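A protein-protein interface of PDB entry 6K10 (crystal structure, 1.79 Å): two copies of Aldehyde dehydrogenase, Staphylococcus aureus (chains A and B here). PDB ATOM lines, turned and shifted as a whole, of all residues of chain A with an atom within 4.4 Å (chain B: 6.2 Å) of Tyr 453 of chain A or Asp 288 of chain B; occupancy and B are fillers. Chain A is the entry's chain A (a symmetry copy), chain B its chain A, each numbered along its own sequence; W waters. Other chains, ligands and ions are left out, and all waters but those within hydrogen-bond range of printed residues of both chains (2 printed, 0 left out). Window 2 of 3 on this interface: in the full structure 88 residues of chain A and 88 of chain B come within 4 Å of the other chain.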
ATOM      1  N   HIS A 449      10.222   9.933   4.255  1.00  0.00           N
ATOM      2  CA  HIS A 449       9.614   8.620   4.082  1.00  0.00           C
ATOM      3  C   HIS A 449       8.336   8.650   3.254  1.00  0.00           C
ATOM      4  O   HIS A 449       7.689   7.609   3.105  1.00  0.00           O
ATOM      5  CB  HIS A 449       9.327   7.990   5.449  1.00  0.00           C
ATOM      6  CG  HIS A 449      10.547   7.815   6.300  1.00  0.00           C
ATOM      7  ND1 HIS A 449      11.534   6.899   6.004  1.00  0.00           N
ATOM      8  CD2 HIS A 449      10.938   8.435   7.438  1.00  0.00           C
ATOM      9  CE1 HIS A 449      12.482   6.966   6.921  1.00  0.00           C
ATOM     10  NE2 HIS A 449      12.144   7.890   7.803  1.00  0.00           N
ATOM     11  N   LEU A 450       7.961   9.800   2.712  1.00  0.00           N
ATOM     12  CA  LEU A 450       6.746   9.936   1.924  1.00  0.00           C
ATOM     13  C   LEU A 450       7.062   9.950   0.437  1.00  0.00           C
ATOM     14  O   LEU A 450       8.182  10.273   0.029  1.00  0.00           O
ATOM     15  CB  LEU A 450       6.011  11.227   2.300  1.00  0.00           C
ATOM     16  CG  LEU A 450       5.673  11.438   3.776  1.00  0.00           C
ATOM     17  CD1 LEU A 450       4.991  12.784   3.977  1.00  0.00           C
ATOM     18  CD2 LEU A 450       4.794  10.309   4.285  1.00  0.00           C
ATOM     19  N   PRO A 451       6.084   9.597  -0.418  1.00  0.00           N
ATOM     20  CA  PRO A 451       6.257   9.801  -1.859  1.00  0.00           C
ATOM     21  C   PRO A 451       6.394  11.286  -2.181  1.00  0.00           C
ATOM     22  O   PRO A 451       5.916  12.112  -1.403  1.00  0.00           O
ATOM     23  CB  PRO A 451       4.973   9.212  -2.465  1.00  0.00           C
ATOM     24  CG  PRO A 451       4.373   8.373  -1.390  1.00  0.00           C
ATOM     25  CD  PRO A 451       4.775   9.004  -0.099  1.00  0.00           C
ATOM     26  N   PRO A 452       7.041  11.629  -3.308  1.00  0.00           N
ATOM     27  CA  PRO A 452       7.648  10.727  -4.300  1.00  0.00           C
ATOM     28  C   PRO A 452       8.926  10.036  -3.808  1.00  0.00           C
ATOM     29  O   PRO A 452       9.688  10.626  -3.043  1.00  0.00           O
ATOM     30  CB  PRO A 452       7.963  11.655  -5.477  1.00  0.00           C
ATOM     31  CG  PRO A 452       8.002  13.022  -4.901  1.00  0.00           C
ATOM     32  CD  PRO A 452       7.066  13.036  -3.744  1.00  0.00           C
ATOM     33  N   TYR A 453       9.147   8.802  -4.261  1.00  0.00           N
ATOM     34  CA  TYR A 453      10.240   7.960  -3.788  1.00  0.00           C
ATOM     35  C   TYR A 453      11.477   8.013  -4.675  1.00  0.00           C
ATOM     36  O   TYR A 453      12.415   7.242  -4.448  1.00  0.00           O
ATOM     37  CB  TYR A 453       9.775   6.507  -3.669  1.00  0.00           C
ATOM     38  CG  TYR A 453       8.753   6.254  -2.587  1.00  0.00           C
ATOM     39  CD1 TYR A 453       8.902   6.803  -1.320  1.00  0.00           C
ATOM     40  CD2 TYR A 453       7.644   5.453  -2.829  1.00  0.00           C
ATOM     41  CE1 TYR A 453       7.966   6.568  -0.325  1.00  0.00           C
ATOM     42  CE2 TYR A 453       6.707   5.212  -1.844  1.00  0.00           C
ATOM     43  CZ  TYR A 453       6.871   5.771  -0.595  1.00  0.00           C
ATOM     44  OH  TYR A 453       5.933   5.527   0.384  1.00  0.00           O
ATOM     45  N   LYS A 454      11.495   8.885  -5.680  1.00  0.00           N
ATOM     46  CA  LYS A 454      12.621   8.950  -6.606  1.00  0.00           C
ATOM     47  C   LYS A 454      13.927   9.174  -5.857  1.00  0.00           C
ATOM     48  O   LYS A 454      14.065  10.138  -5.099  1.00  0.00           O
ATOM     49  CB  LYS A 454      12.392  10.067  -7.627  1.00  0.00           C
ATOM     50  N   GLY A 455      14.876   8.261  -6.057  1.00  0.00           N
ATOM     51  CA  GLY A 455      16.195   8.369  -5.472  1.00  0.00           C
ATOM     52  C   GLY A 455      16.343   7.809  -4.074  1.00  0.00           C
ATOM     53  O   GLY A 455      17.439   7.903  -3.504  1.00  0.00           O
ATOM     54  N   LYS A 456      15.293   7.220  -3.506  1.00  0.00           N
ATOM     55  CA  LYS A 456      15.319   6.778  -2.118  1.00  0.00           C
ATOM     56  C   LYS A 456      15.572   5.285  -1.958  1.00  0.00           C
ATOM     57  O   LYS A 456      15.698   4.816  -0.823  1.00  0.00           O
ATOM     58  CB  LYS A 456      14.005   7.156  -1.421  1.00  0.00           C
ATOM     59  CG  LYS A 456      13.712   8.651  -1.441  1.00  0.00           C
ATOM     60  CD  LYS A 456      12.409   8.993  -0.731  1.00  0.00           C
ATOM     61  CE  LYS A 456      12.152  10.494  -0.766  1.00  0.00           C
ATOM     62  NZ  LYS A 456      10.907  10.878  -0.045  1.00  0.00           N
ATOM     63  N   ASN B  62       6.189  -1.000  -6.485  1.00  0.00           N
ATOM     64  CA  ASN B  62       7.481  -0.402  -6.779  1.00  0.00           C
ATOM     65  C   ASN B  62       8.535  -0.896  -5.789  1.00  0.00           C
ATOM     66  O   ASN B  62       8.230  -1.326  -4.674  1.00  0.00           O
ATOM     67  CB  ASN B  62       7.379   1.124  -6.750  1.00  0.00           C
ATOM     68  CG  ASN B  62       7.168   1.674  -5.350  1.00  0.00           C
ATOM     69  OD1 ASN B  62       8.114   1.816  -4.576  1.00  0.00           O
ATOM     70  ND2 ASN B  62       5.919   1.991  -5.021  1.00  0.00           N
ATOM     71  N   VAL B  64      10.868   0.488  -3.978  1.00  0.00           N
ATOM     72  CA  VAL B  64      11.015   1.133  -2.675  1.00  0.00           C
ATOM     73  C   VAL B  64       9.984   0.583  -1.700  1.00  0.00           C
ATOM     74  O   VAL B  64      10.313   0.163  -0.584  1.00  0.00           O
ATOM     75  CB  VAL B  64      10.902   2.663  -2.812  1.00  0.00           C
ATOM     76  CG1 VAL B  64      10.895   3.317  -1.436  1.00  0.00           C
ATOM     77  CG2 VAL B  64      12.042   3.204  -3.660  1.00  0.00           C
ATOM     78  N   GLU B  65       8.717   0.571  -2.114  1.00  0.00           N
ATOM     79  CA  GLU B  65       7.660   0.035  -1.265  1.00  0.00           C
ATOM     80  C   GLU B  65       7.863  -1.452  -1.007  1.00  0.00           C
ATOM     81  O   GLU B  65       7.646  -1.933   0.112  1.00  0.00           O
ATOM     82  CB  GLU B  65       6.302   0.288  -1.914  1.00  0.00           C
ATOM     83  CG  GLU B  65       5.161   0.474  -0.937  1.00  0.00           C
ATOM     84  CD  GLU B  65       3.820   0.556  -1.635  1.00  0.00           C
ATOM     85  OE1 GLU B  65       3.364   1.684  -1.916  1.00  0.00           O
ATOM     86  OE2 GLU B  65       3.225  -0.506  -1.907  1.00  0.00           O
ATOM     87  N   PHE B 241      -0.364   8.280   3.456  1.00  0.00           N
ATOM     88  CA  PHE B 241       0.733   7.324   3.528  1.00  0.00           C
ATOM     89  C   PHE B 241       0.225   5.924   3.866  1.00  0.00           C
ATOM     90  O   PHE B 241       0.550   4.947   3.182  1.00  0.00           O
ATOM     91  CB  PHE B 241       1.761   7.791   4.565  1.00  0.00           C
ATOM     92  CG  PHE B 241       2.796   6.753   4.895  1.00  0.00           C
ATOM     93  CD1 PHE B 241       3.867   6.529   4.051  1.00  0.00           C
ATOM     94  CD2 PHE B 241       2.700   6.005   6.055  1.00  0.00           C
ATOM     95  CE1 PHE B 241       4.820   5.577   4.358  1.00  0.00           C
ATOM     96  CE2 PHE B 241       3.650   5.053   6.363  1.00  0.00           C
ATOM     97  CZ  PHE B 241       4.710   4.838   5.514  1.00  0.00           C
ATOM     98  N   PHE B 244      -2.791   4.745   0.899  1.00  0.00           N
ATOM     99  CA  PHE B 244      -2.536   4.509  -0.515  1.00  0.00           C
ATOM    100  C   PHE B 244      -1.228   3.777  -0.782  1.00  0.00           C
ATOM    101  O   PHE B 244      -0.915   3.497  -1.944  1.00  0.00           O
ATOM    102  CB  PHE B 244      -2.602   5.840  -1.264  1.00  0.00           C
ATOM    103  CG  PHE B 244      -3.967   6.456  -1.212  1.00  0.00           C
ATOM    104  CD1 PHE B 244      -5.011   5.891  -1.926  1.00  0.00           C
ATOM    105  CD2 PHE B 244      -4.226   7.547  -0.402  1.00  0.00           C
ATOM    106  CE1 PHE B 244      -6.284   6.426  -1.860  1.00  0.00           C
ATOM    107  CE2 PHE B 244      -5.496   8.090  -0.335  1.00  0.00           C
ATOM    108  CZ  PHE B 244      -6.526   7.529  -1.067  1.00  0.00           C
ATOM    109  N   THR B 245      -0.469   3.451   0.261  1.00  0.00           N
ATOM    110  CA  THR B 245       0.515   2.384   0.159  1.00  0.00           C
ATOM    111  C   THR B 245      -0.180   1.092  -0.257  1.00  0.00           C
ATOM    112  O   THR B 245      -1.249   0.755   0.258  1.00  0.00           O
ATOM    113  CB  THR B 245       1.230   2.197   1.501  1.00  0.00           C
ATOM    114  OG1 THR B 245       2.080   3.323   1.755  1.00  0.00           O
ATOM    115  CG2 THR B 245       2.064   0.921   1.507  1.00  0.00           C
ATOM    116  N   PHE B 278       2.159  13.663  -3.531  1.00  0.00           N
ATOM    117  CA  PHE B 278       2.662  12.293  -3.574  1.00  0.00           C
ATOM    118  C   PHE B 278       2.851  11.818  -5.006  1.00  0.00           C
ATOM    119  O   PHE B 278       3.921  11.319  -5.374  1.00  0.00           O
ATOM    120  CB  PHE B 278       1.690  11.349  -2.864  1.00  0.00           C
ATOM    121  CG  PHE B 278       1.800  11.343  -1.367  1.00  0.00           C
ATOM    122  CD1 PHE B 278       2.463  12.352  -0.690  1.00  0.00           C
ATOM    123  CD2 PHE B 278       1.218  10.320  -0.635  1.00  0.00           C
ATOM    124  CE1 PHE B 278       2.549  12.334   0.691  1.00  0.00           C
ATOM    125  CE2 PHE B 278       1.298  10.296   0.742  1.00  0.00           C
ATOM    126  CZ  PHE B 278       1.964  11.304   1.407  1.00  0.00           C
ATOM    127  N   TYR B 279       1.809  11.954  -5.824  1.00  0.00           N
ATOM    128  CA  TYR B 279       1.693  11.198  -7.057  1.00  0.00           C
ATOM    129  C   TYR B 279       1.558  12.045  -8.315  1.00  0.00           C
ATOM    130  O   TYR B 279       1.558  11.478  -9.413  1.00  0.00           O
ATOM    131  CB  TYR B 279       0.489  10.247  -6.973  1.00  0.00           C
ATOM    132  CG  TYR B 279       0.489   9.329  -5.766  1.00  0.00           C
ATOM    133  CD1 TYR B 279       1.515   8.417  -5.561  1.00  0.00           C
ATOM    134  CD2 TYR B 279      -0.553   9.362  -4.843  1.00  0.00           C
ATOM    135  CE1 TYR B 279       1.512   7.568  -4.467  1.00  0.00           C
ATOM    136  CE2 TYR B 279      -0.564   8.517  -3.745  1.00  0.00           C
ATOM    137  CZ  TYR B 279       0.471   7.623  -3.563  1.00  0.00           C
ATOM    138  OH  TYR B 279       0.465   6.781  -2.473  1.00  0.00           O
ATOM    139  N   GLN B 285       0.515   7.654 -13.970  1.00  0.00           N
ATOM    140  CA  GLN B 285       1.899   7.716 -14.418  1.00  0.00           C
ATOM    141  C   GLN B 285       2.900   7.683 -13.270  1.00  0.00           C
ATOM    142  O   GLN B 285       4.107   7.640 -13.524  1.00  0.00           O
ATOM    143  CB  GLN B 285       2.120   8.978 -15.260  1.00  0.00           C
ATOM    144  N   SER B 286       2.438   7.695 -12.022  1.00  0.00           N
ATOM    145  CA  SER B 286       3.355   7.718 -10.886  1.00  0.00           C
ATOM    146  C   SER B 286       4.007   6.351 -10.704  1.00  0.00           C
ATOM    147  O   SER B 286       3.305   5.336 -10.672  1.00  0.00           O
ATOM    148  CB  SER B 286       2.623   8.119  -9.608  1.00  0.00           C
ATOM    149  OG  SER B 286       3.423   7.876  -8.462  1.00  0.00           O
ATOM    150  N   PRO B 287       5.335   6.285 -10.570  1.00  0.00           N
ATOM    151  CA  PRO B 287       5.997   5.004 -10.304  1.00  0.00           C
ATOM    152  C   PRO B 287       5.947   4.578  -8.846  1.00  0.00           C
ATOM    153  O   PRO B 287       6.530   3.547  -8.498  1.00  0.00           O
ATOM    154  CB  PRO B 287       7.438   5.285 -10.739  1.00  0.00           C
ATOM    155  CG  PRO B 287       7.634   6.715 -10.341  1.00  0.00           C
ATOM    156  CD  PRO B 287       6.298   7.401 -10.586  1.00  0.00           C
ATOM    157  N   ASP B 288       5.274   5.349  -7.995  1.00  0.00           N
ATOM    158  CA  ASP B 288       5.218   5.097  -6.562  1.00  0.00           C
ATOM    159  C   ASP B 288       3.875   4.530  -6.127  1.00  0.00           C
ATOM    160  O   ASP B 288       3.626   4.400  -4.924  1.00  0.00           O
ATOM    161  CB  ASP B 288       5.506   6.393  -5.804  1.00  0.00           C
ATOM    162  CG  ASP B 288       6.855   6.981  -6.156  1.00  0.00           C
ATOM    163  OD1 ASP B 288       7.788   6.201  -6.437  1.00  0.00           O
ATOM    164  OD2 ASP B 288       6.973   8.222  -6.181  1.00  0.00           O
ATOM    165  N   TYR B 289       3.007   4.190  -7.073  1.00  0.00           N
ATOM    166  CA  TYR B 289       1.635   3.817  -6.773  1.00  0.00           C
ATOM    167  C   TYR B 289       1.325   2.456  -7.377  1.00  0.00           C
ATOM    168  O   TYR B 289       1.664   2.190  -8.535  1.00  0.00           O
ATOM    169  CB  TYR B 289       0.663   4.877  -7.299  1.00  0.00           C
ATOM    170  CG  TYR B 289      -0.773   4.608  -6.943  1.00  0.00           C
ATOM    171  CD1 TYR B 289      -1.188   4.594  -5.619  1.00  0.00           C
ATOM    172  CD2 TYR B 289      -1.718   4.379  -7.932  1.00  0.00           C
ATOM    173  CE1 TYR B 289      -2.504   4.350  -5.289  1.00  0.00           C
ATOM    174  CE2 TYR B 289      -3.031   4.135  -7.614  1.00  0.00           C
ATOM    175  CZ  TYR B 289      -3.419   4.121  -6.294  1.00  0.00           C
ATOM    176  OH  TYR B 289      -4.731   3.878  -5.985  1.00  0.00           O
ATOM    177  N   GLY B 290       0.667   1.604  -6.590  1.00  0.00           N
ATOM    178  CA  GLY B 290       0.467   0.215  -6.943  1.00  0.00           C
ATOM    179  C   GLY B 290      -0.810  -0.026  -7.728  1.00  0.00           C
ATOM    180  O   GLY B 290      -1.513   0.896  -8.144  1.00  0.00           O
HETATM  181  O   HOH W   1       3.673   3.790  -0.373  1.00  0.00           O
HETATM  182  O   HOH W   2       9.171   9.006  -7.654  1.00  0.00           O
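No position is printed for both chains. Of the 8 pairs that touch across the chains among the printed residues, none has its exchanged pair printed and touching as well.
Water W1 lies within hydrogen-bond range of OE1 of Glu 65 of chain B (2.6 Å), OG1 of Thr 245 of chain B (2.7 Å) and OH of Tyr 453 of chain A (2.9 Å). Water W2 lies within hydrogen-bond range of OD2 of Asp 288 of chain B, N of Lys 454 of chain A and N of Tyr 453 of chain A.
Among the printed residues, pairs that only touch across the chains: Pro 452 of chain A with Asp 288 of chain B, Pro 451 of chain A with Phe 278 of chain B, His 449 of chain A with Phe 241 of chain B, Pro 452 of chain A with Phe 278 of chain B, Tyr 453 of chain A with Val 64 of chain B, Leu 450 of chain A with Phe 241 of chain B and Leu 450 of chain A with Phe 278 of chain B.
Of the printed residues of chain B, Tyr 453 of chain A touches Val 64 and Asp 288. Of chain A, only Pro 452 and Tyr 453 come within 4 Å of Asp 288 of chain B. Of the printed residues of chain B, Leu 450 of chain A touches Phe 241 and Phe 278. Of the printed residues of chain A, Phe 241 of chain B touches His 449 and Leu 450. Thr 245 of chain B touches none of the printed residues of chain A. The nearest residue of chain B that does not touch Tyr 453 of chain A is Asn 62 of chain B (4.1 Å).
The backbone carbonyl oxygen of Phe 241 of chain B is in hydrogen-bond range of the side-chain hydroxyl of Thr 245 of chain B, at 2.6 Å. OD1 of Asn 62 of chain B is in hydrogen-bond range of N of Val 64 of chain B (3.1 Å). O of Pro 452 of chain A sits at hydrogen-bond distance from NZ of Lys 456 of chain A (3.2 Å). The backbone NH of Asp 288 of chain B sits close to the side-chain hydroxyl of Ser 286 of chain B, at 3.2 Å. ND2 of Asn 62 of chain B is in hydrogen-bond range of O of Asp 288 of chain B. The side-chain amino group (NZ) of Lys 456 of chain A is in hydrogen-bond range of the backbone carbonyl oxygen (O) of Leu 450 of chain A (2.8 Å).
OD2 of Asp 288 of chain B is in hydrogen-bond range of N of Tyr 453 of chain A (3.0 Å).
Hydrophobic or aromatic side chains of chain A that line the printed part of chain B: Leu 450, Pro 451, Pro 452 and Tyr 453. Of the 14 printed residues of chain B, 4 touch a printed residue of chain A. Among the printed residues, 8 pairs touch across the chains. Among the printed residues, no Asp or Glu carboxylate lies within 4 Å of a Lys or Arg side-chain nitrogen of the other chain.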
